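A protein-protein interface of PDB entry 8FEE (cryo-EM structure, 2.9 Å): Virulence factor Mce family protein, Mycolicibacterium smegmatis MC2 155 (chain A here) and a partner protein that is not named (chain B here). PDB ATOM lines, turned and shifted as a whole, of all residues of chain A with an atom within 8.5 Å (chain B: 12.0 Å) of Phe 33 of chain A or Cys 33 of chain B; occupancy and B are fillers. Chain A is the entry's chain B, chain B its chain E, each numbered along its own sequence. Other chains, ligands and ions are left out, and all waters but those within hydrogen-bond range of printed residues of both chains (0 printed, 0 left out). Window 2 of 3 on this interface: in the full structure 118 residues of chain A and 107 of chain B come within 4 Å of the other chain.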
ATOM      1  N   ALA A  22       3.764  -8.437   5.243  1.00  0.00           N
ATOM      2  CA  ALA A  22       2.326  -8.398   5.025  1.00  0.00           C
ATOM      3  C   ALA A  22       1.958  -7.373   3.967  1.00  0.00           C
ATOM      4  O   ALA A  22       0.989  -7.574   3.229  1.00  0.00           O
ATOM      5  CB  ALA A  22       1.600  -8.096   6.335  1.00  0.00           C
ATOM      6  N   LEU A  23       2.692  -6.261   3.891  1.00  0.00           N
ATOM      7  CA  LEU A  23       2.464  -5.306   2.815  1.00  0.00           C
ATOM      8  C   LEU A  23       2.766  -5.935   1.462  1.00  0.00           C
ATOM      9  O   LEU A  23       2.063  -5.678   0.481  1.00  0.00           O
ATOM     10  CB  LEU A  23       3.320  -4.060   3.036  1.00  0.00           C
ATOM     11  CG  LEU A  23       3.330  -3.015   1.923  1.00  0.00           C
ATOM     12  CD1 LEU A  23       1.948  -2.412   1.747  1.00  0.00           C
ATOM     13  CD2 LEU A  23       4.356  -1.936   2.221  1.00  0.00           C
ATOM     14  N   PHE A  25       2.384  -9.116   0.780  1.00  0.00           N
ATOM     15  CA  PHE A  25       1.246  -9.993   0.502  1.00  0.00           C
ATOM     16  C   PHE A  25       0.022  -9.203   0.054  1.00  0.00           C
ATOM     17  O   PHE A  25      -0.686  -9.616  -0.869  1.00  0.00           O
ATOM     18  CB  PHE A  25       0.912 -10.847   1.726  1.00  0.00           C
ATOM     19  CG  PHE A  25       1.758 -12.081   1.857  1.00  0.00           C
ATOM     20  CD1 PHE A  25       1.458 -13.218   1.127  1.00  0.00           C
ATOM     21  CD2 PHE A  25       2.840 -12.112   2.718  1.00  0.00           C
ATOM     22  CE1 PHE A  25       2.228 -14.358   1.244  1.00  0.00           C
ATOM     23  CE2 PHE A  25       3.614 -13.249   2.839  1.00  0.00           C
ATOM     24  CZ  PHE A  25       3.306 -14.374   2.101  1.00  0.00           C
ATOM     25  N   VAL A  26      -0.245  -8.065   0.698  1.00  0.00           N
ATOM     26  CA  VAL A  26      -1.390  -7.236   0.327  1.00  0.00           C
ATOM     27  C   VAL A  26      -1.226  -6.691  -1.086  1.00  0.00           C
ATOM     28  O   VAL A  26      -2.178  -6.670  -1.875  1.00  0.00           O
ATOM     29  CB  VAL A  26      -1.582  -6.107   1.358  1.00  0.00           C
ATOM     30  CG1 VAL A  26      -2.511  -5.033   0.822  1.00  0.00           C
ATOM     31  CG2 VAL A  26      -2.123  -6.672   2.659  1.00  0.00           C
ATOM     32  N   VAL A  27      -0.012  -6.256  -1.435  1.00  0.00           N
ATOM     33  CA  VAL A  27       0.216  -5.656  -2.745  1.00  0.00           C
ATOM     34  C   VAL A  27       0.115  -6.703  -3.847  1.00  0.00           C
ATOM     35  O   VAL A  27      -0.529  -6.472  -4.878  1.00  0.00           O
ATOM     36  CB  VAL A  27       1.574  -4.931  -2.769  1.00  0.00           C
ATOM     37  CG1 VAL A  27       1.990  -4.616  -4.193  1.00  0.00           C
ATOM     38  CG2 VAL A  27       1.496  -3.650  -1.959  1.00  0.00           C
ATOM     39  N   GLN A  30      -3.661  -8.708  -4.151  1.00  0.00           N
ATOM     40  CA  GLN A  30      -4.844  -7.913  -4.487  1.00  0.00           C
ATOM     41  C   GLN A  30      -5.904  -7.998  -3.388  1.00  0.00           C
ATOM     42  O   GLN A  30      -7.077  -8.274  -3.641  1.00  0.00           O
ATOM     43  CB  GLN A  30      -5.421  -8.331  -5.843  1.00  0.00           C
ATOM     44  CG  GLN A  30      -4.460  -8.174  -7.013  1.00  0.00           C
ATOM     45  CD  GLN A  30      -4.286  -6.732  -7.454  1.00  0.00           C
ATOM     46  OE1 GLN A  30      -4.898  -5.819  -6.903  1.00  0.00           O
ATOM     47  NE2 GLN A  30      -3.446  -6.523  -8.460  1.00  0.00           N
ATOM     48  N   ILE A  31      -5.476  -7.751  -2.156  1.00  0.00           N
ATOM     49  CA  ILE A  31      -6.355  -7.823  -0.996  1.00  0.00           C
ATOM     50  C   ILE A  31      -7.072  -6.490  -0.835  1.00  0.00           C
ATOM     51  O   ILE A  31      -6.436  -5.429  -0.834  1.00  0.00           O
ATOM     52  CB  ILE A  31      -5.559  -8.177   0.272  1.00  0.00           C
ATOM     53  CG1 ILE A  31      -4.735  -9.445   0.051  1.00  0.00           C
ATOM     54  CG2 ILE A  31      -6.493  -8.344   1.459  1.00  0.00           C
ATOM     55  CD1 ILE A  31      -5.552 -10.642  -0.364  1.00  0.00           C
ATOM     56  N   ARG A  32      -8.394  -6.540  -0.698  1.00  0.00           N
ATOM     57  CA  ARG A  32      -9.206  -5.355  -0.469  1.00  0.00           C
ATOM     58  C   ARG A  32      -9.921  -5.473   0.868  1.00  0.00           C
ATOM     59  O   ARG A  32     -10.212  -6.575   1.340  1.00  0.00           O
ATOM     60  CB  ARG A  32     -10.231  -5.144  -1.590  1.00  0.00           C
ATOM     61  CG  ARG A  32      -9.799  -4.152  -2.661  1.00  0.00           C
ATOM     62  CD  ARG A  32      -8.586  -4.651  -3.421  1.00  0.00           C
ATOM     63  NE  ARG A  32      -8.229  -3.771  -4.525  1.00  0.00           N
ATOM     64  CZ  ARG A  32      -7.271  -4.030  -5.405  1.00  0.00           C
ATOM     65  NH1 ARG A  32      -6.553  -5.137  -5.337  1.00  0.00           N
ATOM     66  NH2 ARG A  32      -7.031  -3.158  -6.378  1.00  0.00           N
ATOM     67  N   PHE A  33     -10.204  -4.325   1.476  1.00  0.00           N
ATOM     68  CA  PHE A  33     -10.774  -4.254   2.816  1.00  0.00           C
ATOM     69  C   PHE A  33     -12.076  -3.460   2.824  1.00  0.00           C
ATOM     70  O   PHE A  33     -12.354  -2.700   3.753  1.00  0.00           O
ATOM     71  CB  PHE A  33      -9.775  -3.647   3.798  1.00  0.00           C
ATOM     72  CG  PHE A  33      -8.388  -4.212   3.680  1.00  0.00           C
ATOM     73  CD1 PHE A  33      -8.036  -5.366   4.356  1.00  0.00           C
ATOM     74  CD2 PHE A  33      -7.433  -3.583   2.897  1.00  0.00           C
ATOM     75  CE1 PHE A  33      -6.761  -5.888   4.248  1.00  0.00           C
ATOM     76  CE2 PHE A  33      -6.158  -4.099   2.786  1.00  0.00           C
ATOM     77  CZ  PHE A  33      -5.823  -5.253   3.462  1.00  0.00           C
ATOM     78  N   ASN A  34     -12.894  -3.626   1.789  1.00  0.00           N
ATOM     79  CA  ASN A  34     -14.144  -2.892   1.657  1.00  0.00           C
ATOM     80  C   ASN A  34     -15.325  -3.850   1.724  1.00  0.00           C
ATOM     81  O   ASN A  34     -15.247  -4.984   1.242  1.00  0.00           O
ATOM     82  CB  ASN A  34     -14.185  -2.103   0.345  1.00  0.00           C
ATOM     83  CG  ASN A  34     -14.026  -2.990  -0.875  1.00  0.00           C
ATOM     84  OD1 ASN A  34     -13.431  -4.064  -0.802  1.00  0.00           O
ATOM     85  ND2 ASN A  34     -14.558  -2.542  -2.004  1.00  0.00           N
ATOM     86  N   ARG A  35     -16.415  -3.389   2.336  1.00  0.00           N
ATOM     87  CA  ARG A  35     -17.628  -4.191   2.420  1.00  0.00           C
ATOM     88  C   ARG A  35     -18.286  -4.277   1.049  1.00  0.00           C
ATOM     89  O   ARG A  35     -18.499  -3.257   0.388  1.00  0.00           O
ATOM     90  CB  ARG A  35     -18.585  -3.587   3.446  1.00  0.00           C
ATOM     91  CG  ARG A  35     -18.121  -3.774   4.881  1.00  0.00           C
ATOM     92  CD  ARG A  35     -18.818  -2.834   5.854  1.00  0.00           C
ATOM     93  NE  ARG A  35     -20.261  -3.037   5.916  1.00  0.00           N
ATOM     94  CZ  ARG A  35     -21.156  -2.232   5.360  1.00  0.00           C
ATOM     95  NH1 ARG A  35     -20.791  -1.168   4.665  1.00  0.00           N
ATOM     96  NH2 ARG A  35     -22.451  -2.500   5.510  1.00  0.00           N
ATOM     97  N   THR A  36     -18.611  -5.492   0.623  1.00  0.00           N
ATOM     98  CA  THR A  36     -19.098  -5.745  -0.726  1.00  0.00           C
ATOM     99  C   THR A  36     -20.468  -6.416  -0.683  1.00  0.00           C
ATOM    100  O   THR A  36     -21.033  -6.678   0.382  1.00  0.00           O
ATOM    101  CB  THR A  36     -18.108  -6.611  -1.512  1.00  0.00           C
ATOM    102  OG1 THR A  36     -17.977  -7.888  -0.879  1.00  0.00           O
ATOM    103  CG2 THR A  36     -16.744  -5.943  -1.584  1.00  0.00           C
ATOM    104  N   LYS A  64     -14.479  -7.630  -7.081  1.00  0.00           N
ATOM    105  CA  LYS A  64     -13.694  -8.740  -7.599  1.00  0.00           C
ATOM    106  C   LYS A  64     -14.610  -9.914  -7.920  1.00  0.00           C
ATOM    107  O   LYS A  64     -15.705 -10.045  -7.368  1.00  0.00           O
ATOM    108  CB  LYS A  64     -12.609  -9.184  -6.604  1.00  0.00           C
ATOM    109  CG  LYS A  64     -11.701  -8.062  -6.114  1.00  0.00           C
ATOM    110  CD  LYS A  64     -10.547  -8.593  -5.283  1.00  0.00           C
ATOM    111  CE  LYS A  64      -9.611  -9.441  -6.122  1.00  0.00           C
ATOM    112  NZ  LYS A  64      -8.458  -9.947  -5.331  1.00  0.00           N
ATOM    113  N   CYS B  33      -7.219   2.391   4.127  1.00  0.00           N
ATOM    114  CA  CYS B  33      -7.655   1.025   4.386  1.00  0.00           C
ATOM    115  C   CYS B  33      -8.975   0.730   3.681  1.00  0.00           C
ATOM    116  O   CYS B  33      -9.065  -0.196   2.876  1.00  0.00           O
ATOM    117  CB  CYS B  33      -7.796   0.783   5.891  1.00  0.00           C
ATOM    118  SG  CYS B  33      -8.234  -0.912   6.336  1.00  0.00           S
ATOM    119  N   GLY B  34     -10.000   1.524   3.997  1.00  0.00           N
ATOM    120  CA  GLY B  34     -11.285   1.350   3.342  1.00  0.00           C
ATOM    121  C   GLY B  34     -11.248   1.710   1.869  1.00  0.00           C
ATOM    122  O   GLY B  34     -11.859   1.030   1.040  1.00  0.00           O
ATOM    123  N   GLN B  35     -10.533   2.778   1.522  1.00  0.00           N
ATOM    124  CA  GLN B  35     -10.444   3.252   0.149  1.00  0.00           C
ATOM    125  C   GLN B  35      -9.259   2.661  -0.605  1.00  0.00           C
ATOM    126  O   GLN B  35      -8.976   3.100  -1.725  1.00  0.00           O
ATOM    127  CB  GLN B  35     -10.362   4.780   0.125  1.00  0.00           C
ATOM    128  CG  GLN B  35      -9.148   5.345   0.842  1.00  0.00           C
ATOM    129  CD  GLN B  35      -9.080   6.858   0.769  1.00  0.00           C
ATOM    130  OE1 GLN B  35      -9.958   7.503   0.196  1.00  0.00           O
ATOM    131  NE2 GLN B  35      -8.034   7.432   1.352  1.00  0.00           N
ATOM    132  N   TRP B  36      -8.554   1.700  -0.011  1.00  0.00           N
ATOM    133  CA  TRP B  36      -7.404   1.081  -0.659  1.00  0.00           C
ATOM    134  C   TRP B  36      -7.821   0.407  -1.958  1.00  0.00           C
ATOM    135  O   TRP B  36      -8.642  -0.515  -1.954  1.00  0.00           O
ATOM    136  CB  TRP B  36      -6.755   0.070   0.285  1.00  0.00           C
ATOM    137  CG  TRP B  36      -5.676  -0.744  -0.355  1.00  0.00           C
ATOM    138  CD1 TRP B  36      -5.792  -2.002  -0.868  1.00  0.00           C
ATOM    139  CD2 TRP B  36      -4.313  -0.353  -0.556  1.00  0.00           C
ATOM    140  NE1 TRP B  36      -4.587  -2.421  -1.374  1.00  0.00           N
ATOM    141  CE2 TRP B  36      -3.662  -1.426  -1.195  1.00  0.00           C
ATOM    142  CE3 TRP B  36      -3.580   0.799  -0.258  1.00  0.00           C
ATOM    143  CZ2 TRP B  36      -2.315  -1.381  -1.541  1.00  0.00           C
ATOM    144  CZ3 TRP B  36      -2.244   0.841  -0.601  1.00  0.00           C
ATOM    145  CH2 TRP B  36      -1.625  -0.241  -1.236  1.00  0.00           C
ATOM    146  N   ARG B  37      -7.257   0.870  -3.072  1.00  0.00           N
ATOM    147  CA  ARG B  37      -7.554   0.317  -4.385  1.00  0.00           C
ATOM    148  C   ARG B  37      -6.371  -0.401  -5.017  1.00  0.00           C
ATOM    149  O   ARG B  37      -6.486  -0.867  -6.154  1.00  0.00           O
ATOM    150  CB  ARG B  37      -8.046   1.422  -5.327  1.00  0.00           C
ATOM    151  CG  ARG B  37      -9.455   1.200  -5.849  1.00  0.00           C
ATOM    152  CD  ARG B  37     -10.476   1.338  -4.734  1.00  0.00           C
ATOM    153  NE  ARG B  37     -11.536   0.344  -4.840  1.00  0.00           N
ATOM    154  CZ  ARG B  37     -12.557   0.247  -4.001  1.00  0.00           C
ATOM    155  NH1 ARG B  37     -12.699   1.083  -2.985  1.00  0.00           N
ATOM    156  NH2 ARG B  37     -13.461  -0.710  -4.187  1.00  0.00           N
ATOM    157  N   GLY B  38      -5.248  -0.506  -4.322  1.00  0.00           N
ATOM    158  CA  GLY B  38      -4.084  -1.201  -4.831  1.00  0.00           C
ATOM    159  C   GLY B  38      -2.873  -0.294  -4.914  1.00  0.00           C
ATOM    160  O   GLY B  38      -2.929   0.901  -4.628  1.00  0.00           O
ATOM    161  N   ILE B  39      -1.756  -0.900  -5.319  1.00  0.00           N
ATOM    162  CA  ILE B  39      -0.509  -0.156  -5.460  1.00  0.00           C
ATOM    163  C   ILE B  39      -0.480   0.650  -6.753  1.00  0.00           C
ATOM    164  O   ILE B  39       0.353   1.553  -6.899  1.00  0.00           O
ATOM    165  CB  ILE B  39       0.690  -1.118  -5.378  1.00  0.00           C
ATOM    166  CG1 ILE B  39       1.992  -0.361  -5.098  1.00  0.00           C
ATOM    167  CG2 ILE B  39       0.811  -1.935  -6.657  1.00  0.00           C
ATOM    168  CD1 ILE B  39       1.945   0.499  -3.857  1.00  0.00           C
ATOM    169  N   ASN B  41      -3.116   2.508  -7.798  1.00  0.00           N
ATOM    170  CA  ASN B  41      -4.012   3.646  -7.651  1.00  0.00           C
ATOM    171  C   ASN B  41      -3.592   4.603  -6.544  1.00  0.00           C
ATOM    172  O   ASN B  41      -4.384   5.469  -6.159  1.00  0.00           O
ATOM    173  CB  ASN B  41      -5.440   3.159  -7.402  1.00  0.00           C
ATOM    174  CG  ASN B  41      -6.070   2.544  -8.634  1.00  0.00           C
ATOM    175  OD1 ASN B  41      -6.879   3.177  -9.312  1.00  0.00           O
ATOM    176  ND2 ASN B  41      -5.700   1.305  -8.933  1.00  0.00           N
ATOM    177  N   VAL B  42      -2.378   4.473  -6.022  1.00  0.00           N
ATOM    178  CA  VAL B  42      -1.889   5.383  -4.989  1.00  0.00           C
ATOM    179  C   VAL B  42      -1.207   6.569  -5.666  1.00  0.00           C
ATOM    180  O   VAL B  42      -0.420   6.377  -6.604  1.00  0.00           O
ATOM    181  CB  VAL B  42      -0.953   4.658  -4.003  1.00  0.00           C
ATOM    182  CG1 VAL B  42       0.152   3.917  -4.736  1.00  0.00           C
ATOM    183  CG2 VAL B  42      -0.365   5.632  -2.996  1.00  0.00           C
ATOM    184  N   PRO B  43      -1.508   7.805  -5.264  1.00  0.00           N
ATOM    185  CA  PRO B  43      -0.845   8.969  -5.875  1.00  0.00           C
ATOM    186  C   PRO B  43       0.634   8.996  -5.518  1.00  0.00           C
ATOM    187  O   PRO B  43       1.002   8.983  -4.342  1.00  0.00           O
ATOM    188  CB  PRO B  43      -1.597  10.164  -5.276  1.00  0.00           C
ATOM    189  CG  PRO B  43      -2.873   9.595  -4.739  1.00  0.00           C
ATOM    190  CD  PRO B  43      -2.540   8.209  -4.297  1.00  0.00           C
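Of the 10 printed residues of chain B, 6 touch a printed residue of chain A.
Hydrophobic or aromatic side chains of chain A that line the printed part of chain B: Val 26, Val 27 and Phe 33.
Among the printed residues, 9 pairs touch across the chains.
Among the printed residues, no Asp or Glu carboxylate lies within 4 Å of a Lys or Arg side-chain nitrogen of the other chain.
ND2 of Asn 34 of chain A lies close to NH2 of Arg 37 of chain B (3.1 Å).
O of Arg 37 of chain B sits close to NH2 of Arg 32 of chain A, at 2.4 Å.
The backbone carbonyl oxygen (O) of Val 26 of chain A sits at hydrogen-bond distance from the backbone NH (N) of Ile 31 of chain A (3.5 Å).
The guanidinium group (NH2) of Arg 32 of chain A lies close to the side-chain amide oxygen (OE1) of Gln 30 of chain A, at 3.5 Å.
Phe 33 of chain A touches just one residue of chain B: Cys 33 (3.6 Å).
Cys 33 of chain B touches just one residue of chain A: Phe 33.
Ile 31 of chain A touches one residue of chain B.
Of the printed residues of chain B, Asn 34 of chain A touches Gly 34 (3.96 Å) and Arg 37 (3.1 Å).
Gly 34 of chain B touches one residue of chain A.
Printed residues of chain A within 4 Å of Gly 38 of chain B: Arg 32 (3.8 Å).
Printed residues of chain B within 4 Å of Arg 32 of chain A: Trp 36, Arg 37 and Gly 38.
Printed residues of chain B within 4 Å of Val 26 of chain A: Trp 36 (3.99 Å).
Printed residues of chain A within 4 Å of Trp 36 of chain B: Val 26 (3.99 Å), Ile 31 (3.5 Å) and Arg 32 (3.9 Å).
Of the printed residues of chain B, Val 27 of chain A touches Ile 39.
Ala 22 of chain A touches none of the printed residues of chain B.
Pro 43 of chain B touches none of the printed residues of chain A.
The nearest residue of chain A that does not touch Cys 33 of chain B is Asn 34 of chain A (5.3 Å).
The nearest printed residue of chain B that does not touch Arg 32 of chain A is Asn 41 of chain B (5.3 Å).
Trp 36 of chain B touches Val 26 of chain A.
Val 27 of chain A touches Ile 39 of chain B (CG1 to CG2, 3.8 Å).
Ile 31 of chain A touches Trp 36 of chain B.
Arg 32 of chain A touches Trp 36 of chain B (CG to O, 3.9 Å).
Arg 32 of chain A touches Gly 38 of chain B (NH2 to N, 3.8 Å).
CB of Phe 33 of chain A touches O of Cys 33 of chain B, at 3.6 Å.
Gly 34 of chain B touches Asn 34 of chain A (O to CB, 3.96 Å).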
